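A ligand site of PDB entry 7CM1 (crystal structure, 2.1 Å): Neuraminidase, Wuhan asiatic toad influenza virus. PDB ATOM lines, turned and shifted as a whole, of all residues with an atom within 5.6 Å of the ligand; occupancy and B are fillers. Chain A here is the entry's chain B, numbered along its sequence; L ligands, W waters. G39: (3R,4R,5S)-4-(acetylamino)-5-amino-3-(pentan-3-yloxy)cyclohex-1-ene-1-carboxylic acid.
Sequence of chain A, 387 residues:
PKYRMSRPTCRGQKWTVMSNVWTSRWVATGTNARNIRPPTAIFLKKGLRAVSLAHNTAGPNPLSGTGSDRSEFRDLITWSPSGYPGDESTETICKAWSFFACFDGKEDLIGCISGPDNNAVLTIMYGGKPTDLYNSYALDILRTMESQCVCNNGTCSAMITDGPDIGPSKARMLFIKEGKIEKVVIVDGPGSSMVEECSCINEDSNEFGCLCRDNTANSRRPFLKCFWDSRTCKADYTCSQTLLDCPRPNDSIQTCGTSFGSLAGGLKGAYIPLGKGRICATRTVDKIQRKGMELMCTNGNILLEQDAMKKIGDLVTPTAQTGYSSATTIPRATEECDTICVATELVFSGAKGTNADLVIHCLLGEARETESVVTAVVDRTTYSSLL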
ATOM      1  N   ARG A  37       0.939  31.156  14.523  1.00  0.00           N
ATOM      2  CA  ARG A  37       2.054  30.203  14.498  1.00  0.00           C
ATOM      3  C   ARG A  37       1.440  28.815  14.537  1.00  0.00           C
ATOM      4  O   ARG A  37       0.499  28.601  15.302  1.00  0.00           O
ATOM      5  CB  ARG A  37       3.014  30.390  15.688  1.00  0.00           C
ATOM      6  CG  ARG A  37       4.220  31.289  15.435  1.00  0.00           C
ATOM      7  CD  ARG A  37       5.494  30.666  16.014  1.00  0.00           C
ATOM      8  NE  ARG A  37       6.010  29.588  15.145  1.00  0.00           N
ATOM      9  CZ  ARG A  37       6.696  28.533  15.578  1.00  0.00           C
ATOM     10  NH1 ARG A  37       6.956  28.373  16.870  1.00  0.00           N
ATOM     11  NH2 ARG A  37       7.126  27.610  14.716  1.00  0.00           N
ATOM     12  N   PRO A  38       1.921  27.857  13.716  1.00  0.00           N
ATOM     13  CA  PRO A  38       2.937  27.976  12.670  1.00  0.00           C
ATOM     14  C   PRO A  38       2.313  27.878  11.289  1.00  0.00           C
ATOM     15  O   PRO A  38       1.792  26.813  10.955  1.00  0.00           O
ATOM     16  CB  PRO A  38       3.850  26.787  12.953  1.00  0.00           C
ATOM     17  CG  PRO A  38       2.926  25.747  13.650  1.00  0.00           C
ATOM     18  CD  PRO A  38       1.612  26.436  13.980  1.00  0.00           C
ATOM     19  N   ASP A  69       2.044  27.910  23.212  1.00  0.00           N
ATOM     20  CA  ASP A  69       1.767  26.828  22.277  1.00  0.00           C
ATOM     21  C   ASP A  69       0.318  26.367  22.394  1.00  0.00           C
ATOM     22  O   ASP A  69      -0.380  26.232  21.393  1.00  0.00           O
ATOM     23  CB  ASP A  69       2.707  25.638  22.529  1.00  0.00           C
ATOM     24  CG  ASP A  69       4.072  25.824  21.912  1.00  0.00           C
ATOM     25  OD1 ASP A  69       4.180  26.526  20.873  1.00  0.00           O
ATOM     26  OD2 ASP A  69       5.047  25.238  22.452  1.00  0.00           O
ATOM     27  N   ARG A  70      -0.125  26.077  23.610  1.00  0.00           N
ATOM     28  CA  ARG A  70      -1.437  25.516  23.871  1.00  0.00           C
ATOM     29  C   ARG A  70      -2.155  26.427  24.839  1.00  0.00           C
ATOM     30  O   ARG A  70      -1.550  26.928  25.792  1.00  0.00           O
ATOM     31  CB  ARG A  70      -1.353  24.086  24.425  1.00  0.00           C
ATOM     32  CG  ARG A  70      -0.602  23.094  23.511  1.00  0.00           C
ATOM     33  CD  ARG A  70      -0.413  21.728  24.192  1.00  0.00           C
ATOM     34  NE  ARG A  70       0.308  21.847  25.457  1.00  0.00           N
ATOM     35  CZ  ARG A  70       1.628  22.018  25.551  1.00  0.00           C
ATOM     36  NH1 ARG A  70       2.191  22.150  26.736  1.00  0.00           N
ATOM     37  NH2 ARG A  70       2.368  22.071  24.455  1.00  0.00           N
ATOM     38  N   ARG A  74      -6.673  29.015  21.524  1.00  0.00           N
ATOM     39  CA  ARG A  74      -6.021  28.622  20.286  1.00  0.00           C
ATOM     40  C   ARG A  74      -7.040  28.172  19.251  1.00  0.00           C
ATOM     41  O   ARG A  74      -8.074  27.577  19.576  1.00  0.00           O
ATOM     42  CB  ARG A  74      -4.999  27.525  20.546  1.00  0.00           C
ATOM     43  CG  ARG A  74      -3.655  28.064  21.007  1.00  0.00           C
ATOM     44  CD  ARG A  74      -2.961  28.779  19.874  1.00  0.00           C
ATOM     45  NE  ARG A  74      -1.656  28.211  19.608  1.00  0.00           N
ATOM     46  CZ  ARG A  74      -0.884  28.532  18.580  1.00  0.00           C
ATOM     47  NH1 ARG A  74      -1.302  29.430  17.690  1.00  0.00           N
ATOM     48  NH2 ARG A  74       0.306  27.956  18.426  1.00  0.00           N
ATOM     49  N   TRP A  97      -5.192  23.611  19.148  1.00  0.00           N
ATOM     50  CA  TRP A  97      -3.794  23.974  19.253  1.00  0.00           C
ATOM     51  C   TRP A  97      -2.897  22.965  18.530  1.00  0.00           C
ATOM     52  O   TRP A  97      -1.673  23.029  18.673  1.00  0.00           O
ATOM     53  CB  TRP A  97      -3.343  24.154  20.712  1.00  0.00           C
ATOM     54  CG  TRP A  97      -3.811  23.140  21.703  1.00  0.00           C
ATOM     55  CD1 TRP A  97      -4.737  23.329  22.687  1.00  0.00           C
ATOM     56  CD2 TRP A  97      -3.341  21.789  21.853  1.00  0.00           C
ATOM     57  NE1 TRP A  97      -4.885  22.186  23.435  1.00  0.00           N
ATOM     58  CE2 TRP A  97      -4.033  21.229  22.941  1.00  0.00           C
ATOM     59  CE3 TRP A  97      -2.401  21.009  21.170  1.00  0.00           C
ATOM     60  CZ2 TRP A  97      -3.825  19.917  23.369  1.00  0.00           C
ATOM     61  CZ3 TRP A  97      -2.192  19.720  21.588  1.00  0.00           C
ATOM     62  CH2 TRP A  97      -2.899  19.179  22.679  1.00  0.00           C
ATOM     63  N   SER A  98      -3.491  22.054  17.773  1.00  0.00           N
ATOM     64  CA  SER A  98      -2.708  21.270  16.816  1.00  0.00           C
ATOM     65  C   SER A  98      -3.662  20.825  15.720  1.00  0.00           C
ATOM     66  O   SER A  98      -4.843  20.599  15.977  1.00  0.00           O
ATOM     67  CB  SER A  98      -2.015  20.089  17.517  1.00  0.00           C
ATOM     68  OG  SER A  98      -1.147  19.392  16.638  1.00  0.00           O
ATOM     69  N   ILE A 141       0.044  15.063  25.702  1.00  0.00           N
ATOM     70  CA  ILE A 141      -0.014  15.992  24.573  1.00  0.00           C
ATOM     71  C   ILE A 141      -0.132  15.226  23.266  1.00  0.00           C
ATOM     72  O   ILE A 141       0.811  15.208  22.452  1.00  0.00           O
ATOM     73  CB  ILE A 141       1.223  16.924  24.542  1.00  0.00           C
ATOM     74  CG1 ILE A 141       1.504  17.515  25.915  1.00  0.00           C
ATOM     75  CG2 ILE A 141       1.011  18.053  23.540  1.00  0.00           C
ATOM     76  CD1 ILE A 141       2.624  18.511  25.898  1.00  0.00           C
ATOM     77  N   LEU A 142      -1.267  14.571  23.052  1.00  0.00           N
ATOM     78  CA  LEU A 142      -1.629  14.140  21.710  1.00  0.00           C
ATOM     79  C   LEU A 142      -1.464  15.318  20.767  1.00  0.00           C
ATOM     80  O   LEU A 142      -1.813  16.448  21.118  1.00  0.00           O
ATOM     81  CB  LEU A 142      -3.072  13.635  21.695  1.00  0.00           C
ATOM     82  CG  LEU A 142      -3.619  12.953  20.455  1.00  0.00           C
ATOM     83  CD1 LEU A 142      -3.001  11.577  20.284  1.00  0.00           C
ATOM     84  CD2 LEU A 142      -5.135  12.861  20.522  1.00  0.00           C
ATOM     85  N   ARG A 143      -0.889  15.068  19.594  1.00  0.00           N
ATOM     86  CA  ARG A 143      -0.525  16.142  18.679  1.00  0.00           C
ATOM     87  C   ARG A 143      -0.366  15.571  17.275  1.00  0.00           C
ATOM     88  O   ARG A 143      -0.252  14.357  17.097  1.00  0.00           O
ATOM     89  CB  ARG A 143       0.750  16.859  19.143  1.00  0.00           C
ATOM     90  CG  ARG A 143       1.912  15.905  19.400  1.00  0.00           C
ATOM     91  CD  ARG A 143       2.931  16.523  20.327  1.00  0.00           C
ATOM     92  NE  ARG A 143       4.160  15.741  20.431  1.00  0.00           N
ATOM     93  CZ  ARG A 143       4.450  14.912  21.435  1.00  0.00           C
ATOM     94  NH1 ARG A 143       3.592  14.755  22.443  1.00  0.00           N
ATOM     95  NH2 ARG A 143       5.594  14.244  21.445  1.00  0.00           N
ATOM     96  N   THR A 144      -0.341  16.460  16.288  1.00  0.00           N
ATOM     97  CA  THR A 144      -0.418  16.034  14.897  1.00  0.00           C
ATOM     98  C   THR A 144       0.538  16.897  14.072  1.00  0.00           C
ATOM     99  O   THR A 144       1.416  17.595  14.604  1.00  0.00           O
ATOM    100  CB  THR A 144      -1.877  16.048  14.434  1.00  0.00           C
ATOM    101  OG1 THR A 144      -1.990  15.527  13.107  1.00  0.00           O
ATOM    102  CG2 THR A 144      -2.442  17.447  14.499  1.00  0.00           C
ATOM    103  N   GLU A 146       0.583  19.567  11.873  1.00  0.00           N
ATOM    104  CA  GLU A 146       0.607  21.007  11.550  1.00  0.00           C
ATOM    105  C   GLU A 146       0.828  21.249  10.068  1.00  0.00           C
ATOM    106  O   GLU A 146       1.456  22.244   9.685  1.00  0.00           O
ATOM    107  CB  GLU A 146       1.651  21.781  12.367  1.00  0.00           C
ATOM    108  CG  GLU A 146       1.911  21.274  13.774  1.00  0.00           C
ATOM    109  CD  GLU A 146       0.694  21.321  14.657  1.00  0.00           C
ATOM    110  OE1 GLU A 146       0.809  20.949  15.836  1.00  0.00           O
ATOM    111  OE2 GLU A 146      -0.386  21.704  14.182  1.00  0.00           O
ATOM    112  N   ASP A 165       7.867  14.881  25.264  1.00  0.00           N
ATOM    113  CA  ASP A 165       8.516  15.561  24.149  1.00  0.00           C
ATOM    114  C   ASP A 165      10.037  15.445  24.185  1.00  0.00           C
ATOM    115  O   ASP A 165      10.696  15.875  23.234  1.00  0.00           O
ATOM    116  CB  ASP A 165       8.089  17.034  24.111  1.00  0.00           C
ATOM    117  CG  ASP A 165       8.863  17.917  25.068  1.00  0.00           C
ATOM    118  OD1 ASP A 165       9.277  17.435  26.158  1.00  0.00           O
ATOM    119  OD2 ASP A 165       9.049  19.109  24.746  1.00  0.00           O
ATOM    120  N   GLU A 196       7.554  13.284  15.350  1.00  0.00           N
ATOM    121  CA  GLU A 196       6.485  14.281  15.410  1.00  0.00           C
ATOM    122  C   GLU A 196       6.569  15.244  14.239  1.00  0.00           C
ATOM    123  O   GLU A 196       7.558  15.308  13.516  1.00  0.00           O
ATOM    124  CB  GLU A 196       6.503  15.028  16.735  1.00  0.00           C
ATOM    125  CG  GLU A 196       7.792  15.701  17.078  1.00  0.00           C
ATOM    126  CD  GLU A 196       7.689  16.279  18.473  1.00  0.00           C
ATOM    127  OE1 GLU A 196       8.455  17.212  18.807  1.00  0.00           O
ATOM    128  OE2 GLU A 196       6.807  15.781  19.214  1.00  0.00           O
ATOM    129  N   GLU A 197       5.463  15.989  14.053  1.00  0.00           N
ATOM    130  CA  GLU A 197       5.361  17.078  13.081  1.00  0.00           C
ATOM    131  C   GLU A 197       5.770  16.633  11.676  1.00  0.00           C
ATOM    132  O   GLU A 197       6.389  17.370  10.905  1.00  0.00           O
ATOM    133  CB  GLU A 197       6.170  18.289  13.546  1.00  0.00           C
ATOM    134  CG  GLU A 197       5.536  19.004  14.718  1.00  0.00           C
ATOM    135  CD  GLU A 197       6.315  20.221  15.163  1.00  0.00           C
ATOM    136  OE1 GLU A 197       7.439  20.415  14.651  1.00  0.00           O
ATOM    137  OE2 GLU A 197       5.794  20.994  16.007  1.00  0.00           O
ATOM    138  N   ARG A 213      10.084  15.373  12.589  1.00  0.00           N
ATOM    139  CA  ARG A 213      10.977  16.009  13.556  1.00  0.00           C
ATOM    140  C   ARG A 213      11.250  15.024  14.682  1.00  0.00           C
ATOM    141  O   ARG A 213      10.329  14.374  15.180  1.00  0.00           O
ATOM    142  CB  ARG A 213      10.318  17.266  14.115  1.00  0.00           C
ATOM    143  CG  ARG A 213      10.867  17.754  15.442  1.00  0.00           C
ATOM    144  CD  ARG A 213      10.129  18.998  15.820  1.00  0.00           C
ATOM    145  NE  ARG A 213      10.669  19.687  16.974  1.00  0.00           N
ATOM    146  CZ  ARG A 213      10.255  20.894  17.342  1.00  0.00           C
ATOM    147  NH1 ARG A 213       9.301  21.510  16.657  1.00  0.00           N
ATOM    148  NH2 ARG A 213      10.780  21.483  18.407  1.00  0.00           N
ATOM    149  N   GLY A 266      14.717  20.483  17.825  1.00  0.00           N
ATOM    150  CA  GLY A 266      14.171  20.018  16.568  1.00  0.00           C
ATOM    151  C   GLY A 266      13.352  21.096  15.897  1.00  0.00           C
ATOM    152  O   GLY A 266      13.047  22.145  16.476  1.00  0.00           O
ATOM    153  N   ARG A 290      17.222  29.241  13.987  1.00  0.00           N
ATOM    154  CA  ARG A 290      16.205  29.063  12.953  1.00  0.00           C
ATOM    155  C   ARG A 290      16.235  30.257  11.991  1.00  0.00           C
ATOM    156  O   ARG A 290      15.317  31.071  11.891  1.00  0.00           O
ATOM    157  CB  ARG A 290      14.830  28.903  13.579  1.00  0.00           C
ATOM    158  CG  ARG A 290      14.685  27.673  14.423  1.00  0.00           C
ATOM    159  CD  ARG A 290      13.350  27.675  15.119  1.00  0.00           C
ATOM    160  NE  ARG A 290      13.132  26.422  15.821  1.00  0.00           N
ATOM    161  CZ  ARG A 290      12.039  26.116  16.490  1.00  0.00           C
ATOM    162  NH1 ARG A 290      11.039  26.984  16.557  1.00  0.00           N
ATOM    163  NH2 ARG A 290      11.947  24.943  17.091  1.00  0.00           N
ATOM    164  N   TYR A 324       9.178  26.850  10.747  1.00  0.00           N
ATOM    165  CA  TYR A 324       8.668  25.634  10.138  1.00  0.00           C
ATOM    166  C   TYR A 324       8.656  25.763   8.616  1.00  0.00           C
ATOM    167  O   TYR A 324       8.724  26.851   8.061  1.00  0.00           O
ATOM    168  CB  TYR A 324       7.251  25.326  10.632  1.00  0.00           C
ATOM    169  CG  TYR A 324       7.159  24.810  12.052  1.00  0.00           C
ATOM    170  CD1 TYR A 324       8.184  25.023  12.961  1.00  0.00           C
ATOM    171  CD2 TYR A 324       6.055  24.084  12.470  1.00  0.00           C
ATOM    172  CE1 TYR A 324       8.101  24.541  14.255  1.00  0.00           C
ATOM    173  CE2 TYR A 324       5.967  23.596  13.758  1.00  0.00           C
ATOM    174  CZ  TYR A 324       6.985  23.832  14.646  1.00  0.00           C
ATOM    175  OH  TYR A 324       6.890  23.329  15.922  1.00  0.00           O
HETATM  176  C1  G39 L   1       8.411  24.705  18.355  1.00  0.00           C
HETATM  177  O1A G39 L   1       9.442  24.098  18.512  1.00  0.00           O
HETATM  178  O1B G39 L   1       8.418  25.831  17.942  1.00  0.00           O
HETATM  179  C2  G39 L   1       7.149  24.051  18.674  1.00  0.00           C
HETATM  180  C3  G39 L   1       5.827  24.770  18.537  1.00  0.00           C
HETATM  181  C4  G39 L   1       4.613  23.818  18.513  1.00  0.00           C
HETATM  182  C5  G39 L   1       4.740  22.709  19.574  1.00  0.00           C
HETATM  183  N5  G39 L   1       3.574  21.848  19.549  1.00  0.00           N
HETATM  184  C10 G39 L   1       2.685  21.746  20.546  1.00  0.00           C
HETATM  185  O10 G39 L   1       2.785  22.401  21.584  1.00  0.00           O
HETATM  186  C11 G39 L   1       1.560  20.778  20.339  1.00  0.00           C
HETATM  187  C6  G39 L   1       6.032  21.907  19.352  1.00  0.00           C
HETATM  188  C7  G39 L   1       7.208  22.788  19.106  1.00  0.00           C
HETATM  189  O7  G39 L   1       6.318  21.073  20.479  1.00  0.00           O
HETATM  190  C8  G39 L   1       6.115  19.657  20.283  1.00  0.00           C
HETATM  191  C9  G39 L   1       6.219  19.257  18.816  1.00  0.00           C
HETATM  192  C81 G39 L   1       4.859  19.192  21.019  1.00  0.00           C
HETATM  193  C82 G39 L   1       4.964  19.318  22.521  1.00  0.00           C
HETATM  194  C91 G39 L   1       5.045  18.449  18.296  1.00  0.00           C
HETATM  195  N4  G39 L   1       3.336  24.537  18.639  1.00  0.00           N
HETATM  196  O   HOH W   1       1.004  23.013  17.176  1.00  0.00           O
HETATM  197  O   HOH W   2       2.417  26.900  17.570  1.00  0.00           O
HETATM  198  O   HOH W   3       2.695  20.096  17.182  1.00  0.00           O
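O10 of the ligand lies within hydrogen-bond range of NH2 of Arg 70. O1A of the ligand lies within salt-bridge range of NH2 of Arg 213, at 2.9 Å. The guanidinium group (NH2) of Arg 290 lies within salt-bridge range of an oxygen (O1A) of the ligand, 3.0 Å away. OD1 of Asp 69 lies within salt-bridge range of N4 of the ligand (3.1 Å). NH1 of Arg 37 is in salt-bridge range of O1B of the ligand, 3.1 Å away.
The side-chain hydroxyl (OH) of Tyr 324 lies within hydrogen-bond range of the guanidinium group (NH1) of Arg 213, 3.1 Å away. OH of Tyr 324 sits at hydrogen-bond distance from OE2 of Glu 197. The side-chain carboxylate (OE1) of Glu 197 lies within salt-bridge range of the guanidinium group (NH1) of Arg 213. The guanidinium group (NH2) of Arg 213 sits at hydrogen-bond distance from the backbone carbonyl oxygen (O) of Gly 266 (3.1 Å). The backbone carbonyl oxygen of Gly 266 is in hydrogen-bond range of the guanidinium group of Arg 290, at 3.1 Å. OE2 of Glu 196 lies within salt-bridge range of NE of Arg 143 (2.9 Å). The guanidinium group (NE) of Arg 74 is in hydrogen-bond range of the backbone carbonyl oxygen (O) of Asp 69, at 3.0 Å. The backbone carbonyl oxygen of Ile 141 sits at hydrogen-bond distance from the guanidinium group of Arg 143, 2.8 Å away.
CD of Arg 143 touches C81 of the ligand, at 3.4 Å. Glu 196 touches the ligand (OE1 to C9, 3.0 Å). Glu 197 touches the ligand. Tyr 324 touches the ligand. Nine residues have an atom within 4 Å of the ligand: Arg 37, Asp 69, Arg 70, Arg 143, Glu 196, Glu 197, Arg 213, Arg 290 and Tyr 324. The nearest printed residue that does not touch the ligand is Trp 97 (4.1 Å).
Water W2 lies within hydrogen-bond range of NH2 of Arg 74 (2.5 Å), N4 of the ligand (2.8 Å) and O of Arg 37 (3.4 Å). Water W3 lies within hydrogen-bond range of the side-chain carboxylate of Glu 146 (2.5 Å), a nitrogen (N5) of the ligand (3.1 Å) and the side-chain carboxylate of Glu 197 (3.4 Å). Water W1 lies within hydrogen-bond range of the side-chain carboxylate of Glu 146, the backbone carbonyl oxygen of Trp 97 and a nitrogen (N4) of the ligand.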
